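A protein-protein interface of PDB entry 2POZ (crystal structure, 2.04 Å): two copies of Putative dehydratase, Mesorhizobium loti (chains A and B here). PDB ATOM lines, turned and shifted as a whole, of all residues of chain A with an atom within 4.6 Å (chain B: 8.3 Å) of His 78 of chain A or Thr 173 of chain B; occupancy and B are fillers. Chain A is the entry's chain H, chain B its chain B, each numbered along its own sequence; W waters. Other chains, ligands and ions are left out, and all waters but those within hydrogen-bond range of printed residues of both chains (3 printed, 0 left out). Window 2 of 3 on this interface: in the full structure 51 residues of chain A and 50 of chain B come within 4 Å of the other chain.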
ATOM      1  N   PHE A  59      14.995  -0.360   5.978  1.00  0.00           N
ATOM      2  CA  PHE A  59      13.551  -0.514   5.824  1.00  0.00           C
ATOM      3  C   PHE A  59      12.699  -1.110   6.952  1.00  0.00           C
ATOM      4  O   PHE A  59      11.473  -0.995   6.906  1.00  0.00           O
ATOM      5  CB  PHE A  59      13.270  -1.362   4.576  1.00  0.00           C
ATOM      6  CG  PHE A  59      13.890  -0.838   3.308  1.00  0.00           C
ATOM      7  CD1 PHE A  59      13.416   0.323   2.709  1.00  0.00           C
ATOM      8  CD2 PHE A  59      14.920  -1.543   2.684  1.00  0.00           C
ATOM      9  CE1 PHE A  59      13.950   0.775   1.501  1.00  0.00           C
ATOM     10  CE2 PHE A  59      15.462  -1.100   1.478  1.00  0.00           C
ATOM     11  CZ  PHE A  59      14.974   0.062   0.884  1.00  0.00           C
ATOM     12  N   THR A  74       8.448  -1.931  -1.019  1.00  0.00           N
ATOM     13  CA  THR A  74       9.366  -0.860  -0.654  1.00  0.00           C
ATOM     14  C   THR A  74      10.826  -1.256  -0.857  1.00  0.00           C
ATOM     15  O   THR A  74      11.625  -0.472  -1.384  1.00  0.00           O
ATOM     16  CB  THR A  74       9.179  -0.444   0.813  1.00  0.00           C
ATOM     17  OG1 THR A  74       7.840   0.024   1.011  1.00  0.00           O
ATOM     18  CG2 THR A  74      10.159   0.658   1.171  1.00  0.00           C
ATOM     19  N   MET A  75      11.178  -2.460  -0.416  1.00  0.00           N
ATOM     20  CA  MET A  75      12.546  -2.943  -0.557  1.00  0.00           C
ATOM     21  C   MET A  75      12.878  -3.119  -2.034  1.00  0.00           C
ATOM     22  O   MET A  75      14.002  -2.869  -2.456  1.00  0.00           O
ATOM     23  CB  MET A  75      12.736  -4.269   0.189  1.00  0.00           C
ATOM     24  CG  MET A  75      12.564  -4.133   1.697  1.00  0.00           C
ATOM     25  SD  MET A  75      13.058  -5.714   2.684  1.00  0.00           S
ATOM     26  CE  MET A  75      11.582  -6.866   2.185  1.00  0.00           C
ATOM     27  N   TYR A  76      11.889  -3.534  -2.816  1.00  0.00           N
ATOM     28  CA  TYR A  76      12.092  -3.729  -4.245  1.00  0.00           C
ATOM     29  C   TYR A  76      12.294  -2.386  -4.949  1.00  0.00           C
ATOM     30  O   TYR A  76      13.244  -2.210  -5.712  1.00  0.00           O
ATOM     31  CB  TYR A  76      10.889  -4.439  -4.872  1.00  0.00           C
ATOM     32  CG  TYR A  76      11.070  -4.707  -6.351  1.00  0.00           C
ATOM     33  CD1 TYR A  76      11.651  -5.894  -6.799  1.00  0.00           C
ATOM     34  CD2 TYR A  76      10.731  -3.739  -7.302  1.00  0.00           C
ATOM     35  CE1 TYR A  76      11.900  -6.113  -8.159  1.00  0.00           C
ATOM     36  CE2 TYR A  76      10.979  -3.948  -8.669  1.00  0.00           C
ATOM     37  CZ  TYR A  76      11.564  -5.136  -9.085  1.00  0.00           C
ATOM     38  OH  TYR A  76      11.826  -5.343 -10.425  1.00  0.00           O
ATOM     39  N   ASP A  77      11.392  -1.445  -4.685  1.00  0.00           N
ATOM     40  CA  ASP A  77      11.428  -0.123  -5.308  1.00  0.00           C
ATOM     41  C   ASP A  77      12.589   0.777  -4.917  1.00  0.00           C
ATOM     42  O   ASP A  77      13.079   1.556  -5.741  1.00  0.00           O
ATOM     43  CB  ASP A  77      10.150   0.664  -4.993  1.00  0.00           C
ATOM     44  CG  ASP A  77       8.901   0.049  -5.597  1.00  0.00           C
ATOM     45  OD1 ASP A  77       9.015  -0.944  -6.349  1.00  0.00           O
ATOM     46  OD2 ASP A  77       7.800   0.577  -5.317  1.00  0.00           O
ATOM     47  N   HIS A  78      13.034   0.670  -3.671  1.00  0.00           N
ATOM     48  CA  HIS A  78      14.060   1.573  -3.186  1.00  0.00           C
ATOM     49  C   HIS A  78      15.410   1.039  -2.746  1.00  0.00           C
ATOM     50  O   HIS A  78      16.184   1.764  -2.122  1.00  0.00           O
ATOM     51  CB  HIS A  78      13.438   2.426  -2.081  1.00  0.00           C
ATOM     52  CG  HIS A  78      12.138   3.052  -2.487  1.00  0.00           C
ATOM     53  ND1 HIS A  78      12.042   3.968  -3.514  1.00  0.00           N
ATOM     54  CD2 HIS A  78      10.873   2.858  -2.042  1.00  0.00           C
ATOM     55  CE1 HIS A  78      10.778   4.310  -3.684  1.00  0.00           C
ATOM     56  NE2 HIS A  78      10.048   3.652  -2.804  1.00  0.00           N
ATOM     57  N   SER A  79      15.706  -0.212  -3.074  1.00  0.00           N
ATOM     58  CA  SER A  79      17.007  -0.778  -2.732  1.00  0.00           C
ATOM     59  C   SER A  79      17.948  -0.509  -3.915  1.00  0.00           C
ATOM     60  O   SER A  79      19.175  -0.542  -3.781  1.00  0.00           O
ATOM     61  CB  SER A  79      16.882  -2.284  -2.518  1.00  0.00           C
ATOM     62  OG  SER A  79      16.450  -2.919  -3.704  1.00  0.00           O
ATOM     63  N   PHE A  80      17.326  -0.220  -5.059  1.00  0.00           N
ATOM     64  CA  PHE A  80      17.974   0.027  -6.348  1.00  0.00           C
ATOM     65  C   PHE A  80      18.400  -1.291  -6.986  1.00  0.00           C
ATOM     66  O   PHE A  80      18.028  -1.583  -8.123  1.00  0.00           O
ATOM     67  CB  PHE A  80      19.203   0.941  -6.242  1.00  0.00           C
ATOM     68  CG  PHE A  80      19.684   1.454  -7.587  1.00  0.00           C
ATOM     69  CD1 PHE A  80      19.072   2.556  -8.182  1.00  0.00           C
ATOM     70  CD2 PHE A  80      20.693   0.794  -8.286  1.00  0.00           C
ATOM     71  CE1 PHE A  80      19.455   2.996  -9.461  1.00  0.00           C
ATOM     72  CE2 PHE A  80      21.085   1.219  -9.561  1.00  0.00           C
ATOM     73  CZ  PHE A  80      20.464   2.322 -10.152  1.00  0.00           C
ATOM     74  N   TYR B  41      26.039   3.058  -3.777  1.00  0.00           N
ATOM     75  CA  TYR B  41      24.768   3.684  -3.458  1.00  0.00           C
ATOM     76  C   TYR B  41      23.739   2.570  -3.440  1.00  0.00           C
ATOM     77  O   TYR B  41      24.056   1.418  -3.749  1.00  0.00           O
ATOM     78  CB  TYR B  41      24.415   4.739  -4.512  1.00  0.00           C
ATOM     79  CG  TYR B  41      24.444   4.207  -5.928  1.00  0.00           C
ATOM     80  CD1 TYR B  41      23.306   3.651  -6.512  1.00  0.00           C
ATOM     81  CD2 TYR B  41      25.630   4.206  -6.665  1.00  0.00           C
ATOM     82  CE1 TYR B  41      23.351   3.101  -7.799  1.00  0.00           C
ATOM     83  CE2 TYR B  41      25.684   3.660  -7.950  1.00  0.00           C
ATOM     84  CZ  TYR B  41      24.543   3.109  -8.508  1.00  0.00           C
ATOM     85  OH  TYR B  41      24.604   2.560  -9.764  1.00  0.00           O
ATOM     86  N   GLY B  42      22.508   2.908  -3.080  1.00  0.00           N
ATOM     87  CA  GLY B  42      21.475   1.898  -3.004  1.00  0.00           C
ATOM     88  C   GLY B  42      21.669   1.116  -1.717  1.00  0.00           C
ATOM     89  O   GLY B  42      22.445   1.522  -0.849  1.00  0.00           O
ATOM     90  N   VAL B  43      20.975  -0.006  -1.590  1.00  0.00           N
ATOM     91  CA  VAL B  43      21.076  -0.833  -0.396  1.00  0.00           C
ATOM     92  C   VAL B  43      21.846  -2.114  -0.704  1.00  0.00           C
ATOM     93  O   VAL B  43      21.412  -2.919  -1.534  1.00  0.00           O
ATOM     94  CB  VAL B  43      19.662  -1.184   0.136  1.00  0.00           C
ATOM     95  CG1 VAL B  43      19.757  -2.007   1.408  1.00  0.00           C
ATOM     96  CG2 VAL B  43      18.879   0.101   0.405  1.00  0.00           C
ATOM     97  N   GLY B  44      22.994  -2.291  -0.052  1.00  0.00           N
ATOM     98  CA  GLY B  44      23.788  -3.487  -0.281  1.00  0.00           C
ATOM     99  C   GLY B  44      25.291  -3.330  -0.116  1.00  0.00           C
ATOM    100  O   GLY B  44      26.045  -4.262  -0.388  1.00  0.00           O
ATOM    101  N   LEU B 161      11.596  12.423 -12.641  1.00  0.00           N
ATOM    102  CA  LEU B 161      10.566  11.759 -11.837  1.00  0.00           C
ATOM    103  C   LEU B 161      10.953  11.568 -10.377  1.00  0.00           C
ATOM    104  O   LEU B 161      10.120  11.169  -9.568  1.00  0.00           O
ATOM    105  CB  LEU B 161      10.232  10.371 -12.406  1.00  0.00           C
ATOM    106  CG  LEU B 161      10.017  10.162 -13.907  1.00  0.00           C
ATOM    107  CD1 LEU B 161       9.770   8.680 -14.176  1.00  0.00           C
ATOM    108  CD2 LEU B 161       8.850  10.985 -14.392  1.00  0.00           C
ATOM    109  N   LEU B 169      18.526  10.385  -3.727  1.00  0.00           N
ATOM    110  CA  LEU B 169      17.304  10.540  -4.504  1.00  0.00           C
ATOM    111  C   LEU B 169      16.369   9.360  -4.310  1.00  0.00           C
ATOM    112  O   LEU B 169      16.819   8.217  -4.221  1.00  0.00           O
ATOM    113  CB  LEU B 169      17.617  10.651  -6.001  1.00  0.00           C
ATOM    114  CG  LEU B 169      18.342  11.857  -6.593  1.00  0.00           C
ATOM    115  CD1 LEU B 169      18.599  11.597  -8.081  1.00  0.00           C
ATOM    116  CD2 LEU B 169      17.500  13.110  -6.408  1.00  0.00           C
ATOM    117  N   GLN B 170      15.068   9.639  -4.252  1.00  0.00           N
ATOM    118  CA  GLN B 170      14.067   8.587  -4.122  1.00  0.00           C
ATOM    119  C   GLN B 170      13.354   8.497  -5.465  1.00  0.00           C
ATOM    120  O   GLN B 170      12.809   9.498  -5.953  1.00  0.00           O
ATOM    121  CB  GLN B 170      13.044   8.905  -3.025  1.00  0.00           C
ATOM    122  CG  GLN B 170      11.998   7.796  -2.876  1.00  0.00           C
ATOM    123  CD  GLN B 170      11.166   7.923  -1.620  1.00  0.00           C
ATOM    124  OE1 GLN B 170      11.706   8.043  -0.520  1.00  0.00           O
ATOM    125  NE2 GLN B 170       9.844   7.892  -1.773  1.00  0.00           N
ATOM    126  N   HIS B 171      13.356   7.311  -6.070  1.00  0.00           N
ATOM    127  CA  HIS B 171      12.703   7.155  -7.363  1.00  0.00           C
ATOM    128  C   HIS B 171      11.231   6.798  -7.233  1.00  0.00           C
ATOM    129  O   HIS B 171      10.651   6.934  -6.160  1.00  0.00           O
ATOM    130  CB  HIS B 171      13.471   6.142  -8.218  1.00  0.00           C
ATOM    131  CG  HIS B 171      14.884   6.564  -8.492  1.00  0.00           C
ATOM    132  ND1 HIS B 171      15.956   6.115  -7.748  1.00  0.00           N
ATOM    133  CD2 HIS B 171      15.388   7.484  -9.351  1.00  0.00           C
ATOM    134  CE1 HIS B 171      17.055   6.739  -8.134  1.00  0.00           C
ATOM    135  NE2 HIS B 171      16.739   7.576  -9.105  1.00  0.00           N
ATOM    136  N   VAL B 172      10.623   6.357  -8.328  1.00  0.00           N
ATOM    137  CA  VAL B 172       9.204   6.035  -8.333  1.00  0.00           C
ATOM    138  C   VAL B 172       8.770   4.893  -7.424  1.00  0.00           C
ATOM    139  O   VAL B 172       9.434   3.863  -7.327  1.00  0.00           O
ATOM    140  CB  VAL B 172       8.720   5.722  -9.763  1.00  0.00           C
ATOM    141  CG1 VAL B 172       7.250   5.332  -9.740  1.00  0.00           C
ATOM    142  CG2 VAL B 172       8.933   6.937 -10.658  1.00  0.00           C
ATOM    143  N   THR B 173       7.638   5.085  -6.758  1.00  0.00           N
ATOM    144  CA  THR B 173       7.082   4.052  -5.889  1.00  0.00           C
ATOM    145  C   THR B 173       5.999   3.314  -6.674  1.00  0.00           C
ATOM    146  O   THR B 173       5.083   3.934  -7.205  1.00  0.00           O
ATOM    147  CB  THR B 173       6.432   4.654  -4.620  1.00  0.00           C
ATOM    148  OG1 THR B 173       7.446   5.188  -3.765  1.00  0.00           O
ATOM    149  CG2 THR B 173       5.648   3.583  -3.861  1.00  0.00           C
ATOM    150  N   ARG B 174       6.117   1.995  -6.753  1.00  0.00           N
ATOM    151  CA  ARG B 174       5.127   1.179  -7.447  1.00  0.00           C
ATOM    152  C   ARG B 174       4.727   1.672  -8.844  1.00  0.00           C
ATOM    153  O   ARG B 174       3.549   1.631  -9.218  1.00  0.00           O
ATOM    154  CB  ARG B 174       3.876   1.031  -6.561  1.00  0.00           C
ATOM    155  CG  ARG B 174       4.110   0.205  -5.298  1.00  0.00           C
ATOM    156  CD  ARG B 174       2.839   0.055  -4.458  1.00  0.00           C
ATOM    157  NE  ARG B 174       2.561   1.228  -3.633  1.00  0.00           N
ATOM    158  CZ  ARG B 174       3.232   1.541  -2.528  1.00  0.00           C
ATOM    159  NH1 ARG B 174       4.224   0.768  -2.108  1.00  0.00           N
ATOM    160  NH2 ARG B 174       2.910   2.622  -1.836  1.00  0.00           N
ATOM    161  N   ARG B 175       5.713   2.136  -9.610  1.00  0.00           N
ATOM    162  CA  ARG B 175       5.488   2.609 -10.976  1.00  0.00           C
ATOM    163  C   ARG B 175       4.283   3.533 -11.135  1.00  0.00           C
ATOM    164  O   ARG B 175       3.668   3.572 -12.203  1.00  0.00           O
ATOM    165  CB  ARG B 175       5.321   1.411 -11.912  1.00  0.00           C
ATOM    166  CG  ARG B 175       6.490   0.449 -11.874  1.00  0.00           C
ATOM    167  CD  ARG B 175       6.146  -0.859 -12.560  1.00  0.00           C
ATOM    168  NE  ARG B 175       7.230  -1.827 -12.439  1.00  0.00           N
ATOM    169  CZ  ARG B 175       7.102  -3.126 -12.696  1.00  0.00           C
ATOM    170  NH1 ARG B 175       5.934  -3.616 -13.085  1.00  0.00           N
ATOM    171  NH2 ARG B 175       8.149  -3.932 -12.577  1.00  0.00           N
ATOM    172  N   SER B 176       3.953   4.280 -10.083  1.00  0.00           N
ATOM    173  CA  SER B 176       2.814   5.195 -10.130  1.00  0.00           C
ATOM    174  C   SER B 176       3.169   6.593  -9.666  1.00  0.00           C
ATOM    175  O   SER B 176       3.993   6.777  -8.765  1.00  0.00           O
ATOM    176  CB  SER B 176       1.665   4.677  -9.262  1.00  0.00           C
ATOM    177  OG  SER B 176       1.155   3.456  -9.764  1.00  0.00           O
ATOM    178  N   MET B 177       2.525   7.573 -10.290  1.00  0.00           N
ATOM    179  CA  MET B 177       2.720   8.976  -9.970  1.00  0.00           C
ATOM    180  C   MET B 177       1.419   9.710 -10.229  1.00  0.00           C
ATOM    181  O   MET B 177       0.669   9.353 -11.138  1.00  0.00           O
ATOM    182  CB  MET B 177       3.806   9.583 -10.851  1.00  0.00           C
ATOM    183  CG  MET B 177       5.217   9.275 -10.422  1.00  0.00           C
ATOM    184  SD  MET B 177       6.467  10.039 -11.678  1.00  0.00           S
ATOM    185  CE  MET B 177       6.367  11.894 -11.123  1.00  0.00           C
ATOM    186  N   SER B 178       1.152  10.736  -9.432  1.00  0.00           N
ATOM    187  CA  SER B 178      -0.057  11.523  -9.614  1.00  0.00           C
ATOM    188  C   SER B 178       0.095  12.345 -10.889  1.00  0.00           C
ATOM    189  O   SER B 178       1.205  12.508 -11.413  1.00  0.00           O
ATOM    190  CB  SER B 178      -0.266  12.460  -8.425  1.00  0.00           C
ATOM    191  OG  SER B 178       0.748  13.451  -8.377  1.00  0.00           O
ATOM    192  N   GLY B 209      11.102   4.183 -14.545  1.00  0.00           N
ATOM    193  CA  GLY B 209       9.871   4.773 -15.040  1.00  0.00           C
ATOM    194  C   GLY B 209       8.570   4.323 -14.402  1.00  0.00           C
ATOM    195  O   GLY B 209       8.526   3.894 -13.252  1.00  0.00           O
ATOM    196  N   LEU B 210       7.497   4.435 -15.175  1.00  0.00           N
ATOM    197  CA  LEU B 210       6.154   4.081 -14.727  1.00  0.00           C
ATOM    198  C   LEU B 210       5.740   2.803 -15.451  1.00  0.00           C
ATOM    199  O   LEU B 210       6.587   2.002 -15.834  1.00  0.00           O
ATOM    200  CB  LEU B 210       5.195   5.218 -15.098  1.00  0.00           C
ATOM    201  CG  LEU B 210       5.701   6.626 -14.745  1.00  0.00           C
ATOM    202  CD1 LEU B 210       4.803   7.697 -15.355  1.00  0.00           C
ATOM    203  CD2 LEU B 210       5.749   6.766 -13.227  1.00  0.00           C
ATOM    204  N   ARG B 258      22.002  -1.697 -14.688  1.00  0.00           N
ATOM    205  CA  ARG B 258      21.596  -2.871 -13.928  1.00  0.00           C
ATOM    206  C   ARG B 258      21.527  -4.153 -14.755  1.00  0.00           C
ATOM    207  O   ARG B 258      20.610  -4.961 -14.599  1.00  0.00           O
ATOM    208  CB  ARG B 258      20.257  -2.605 -13.225  1.00  0.00           C
ATOM    209  CG  ARG B 258      20.431  -1.765 -11.964  1.00  0.00           C
ATOM    210  CD  ARG B 258      19.118  -1.387 -11.297  1.00  0.00           C
ATOM    211  NE  ARG B 258      18.465  -0.269 -11.975  1.00  0.00           N
ATOM    212  CZ  ARG B 258      17.512   0.483 -11.429  1.00  0.00           C
ATOM    213  NH1 ARG B 258      17.094   0.247 -10.189  1.00  0.00           N
ATOM    214  NH2 ARG B 258      16.978   1.478 -12.123  1.00  0.00           N
HETATM  215  O   HOH W   1      11.939   2.844  -7.925  1.00  0.00           O
HETATM  216  O   HOH W   2      14.462   4.931  -4.901  1.00  0.00           O
HETATM  217  O   HOH W   3       7.108   0.826  -2.643  1.00  0.00           O
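The guanidinium group of Arg 258 of chain B sits at hydrogen-bond distance from the backbone carbonyl oxygen of Phe 80 of chain A (2.9 Å). The backbone NH of Arg 174 of chain B is in hydrogen-bond range of the side-chain carboxylate of Asp 77 of chain A (2.6 Å). The backbone NH of Val 43 of chain B lies within hydrogen-bond range of the backbone carbonyl oxygen of Ser 79 of chain A (2.9 Å). The side-chain hydroxyl (OG1) of Thr 173 of chain B is in hydrogen-bond range of a ring nitrogen (NE2) of His 78 of chain A, at 3.2 Å.
O of Met 75 of chain A sits at hydrogen-bond distance from OG of Ser 79 of chain A (2.7 Å). The backbone carbonyl oxygen (O) of Arg 174 of chain B sits at hydrogen-bond distance from the side-chain hydroxyl (OG) of Ser 176 of chain B (3.1 Å).
Val 43 of chain B touches Phe 59 of chain A (CG2 to CE2, 3.8 Å). OD2 of Asp 77 of chain A touches C of Thr 173 of chain B, 3.5 Å away. CE1 of His 78 of chain A touches CG of Gln 170 of chain B (3.8 Å). His 78 of chain A touches His 171 of chain B (CE1 to O, 3.6 Å). CE1 of His 78 of chain A touches O of Val 172 of chain B (3.9 Å). Ser 79 of chain A touches Gly 42 of chain B. Phe 80 of chain A touches Tyr 41 of chain B (CE2 to CE1, 3.4 Å).
Of the printed residues of chain B, Phe 59 of chain A touches Val 43. Met 75 of chain A touches none of the printed residues of chain B. Printed residues of chain B within 4 Å of His 78 of chain A: Gln 170 (3.8 Å), His 171 (3.6 Å), Val 172 (3.9 Å) and Thr 173 (3.2 Å). Of chain B, only Gly 42 (3.4 Å) and Val 43 (2.9 Å) come within 4 Å of Ser 79 of chain A. Of the printed residues of chain B, Phe 80 of chain A touches Tyr 41 and Arg 258. Leu 169 of chain B touches none of the printed residues of chain A. Printed residues of chain A within 4 Å of Gln 170 of chain B: His 78 (3.8 Å). Of the printed residues of chain A, His 171 of chain B touches His 78. Printed residues of chain A within 4 Å of Val 172 of chain B: His 78 (3.9 Å). Thr 173 of chain B touches just these residues of chain A: Asp 77 and His 78. The nearest printed residue of chain A that does not touch Arg 258 of chain B is Asp 77 of chain A (6.1 Å).
Of the 18 printed residues of chain B, 9 touch a printed residue of chain A. Printed residues of chain B that touch a printed residue of chain A: Tyr 41, Gly 42, Val 43, Gln 170, His 171, Val 172, Thr 173, Arg 174 and Arg 258. Along chain A the printed residues that touch a printed residue of chain B span positions 59 to 80. Among the printed residues, 11 pairs touch across the chains.
No position is printed for both chains. Of the 11 pairs that touch across the chains among the printed residues, none has its exchanged pair printed and touching as well.
Water W1 lies within hydrogen-bond range of the backbone carbonyl oxygen of Val 172 of chain B (2.8 Å) and the backbone carbonyl oxygen of Asp 77 of chain A (2.8 Å). Water W3 lies within hydrogen-bond range of the side-chain carboxylate (OD2) of Asp 77 of chain A (2.8 Å), the guanidinium group (NH1) of Arg 174 of chain B (2.9 Å) and the backbone NH (N) of Thr 74 of chain A (3.5 Å). Water W2 bridges N of His 171 of chain B (2.9 Å) and ND1 of His 78 of chain A (3.0 Å).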
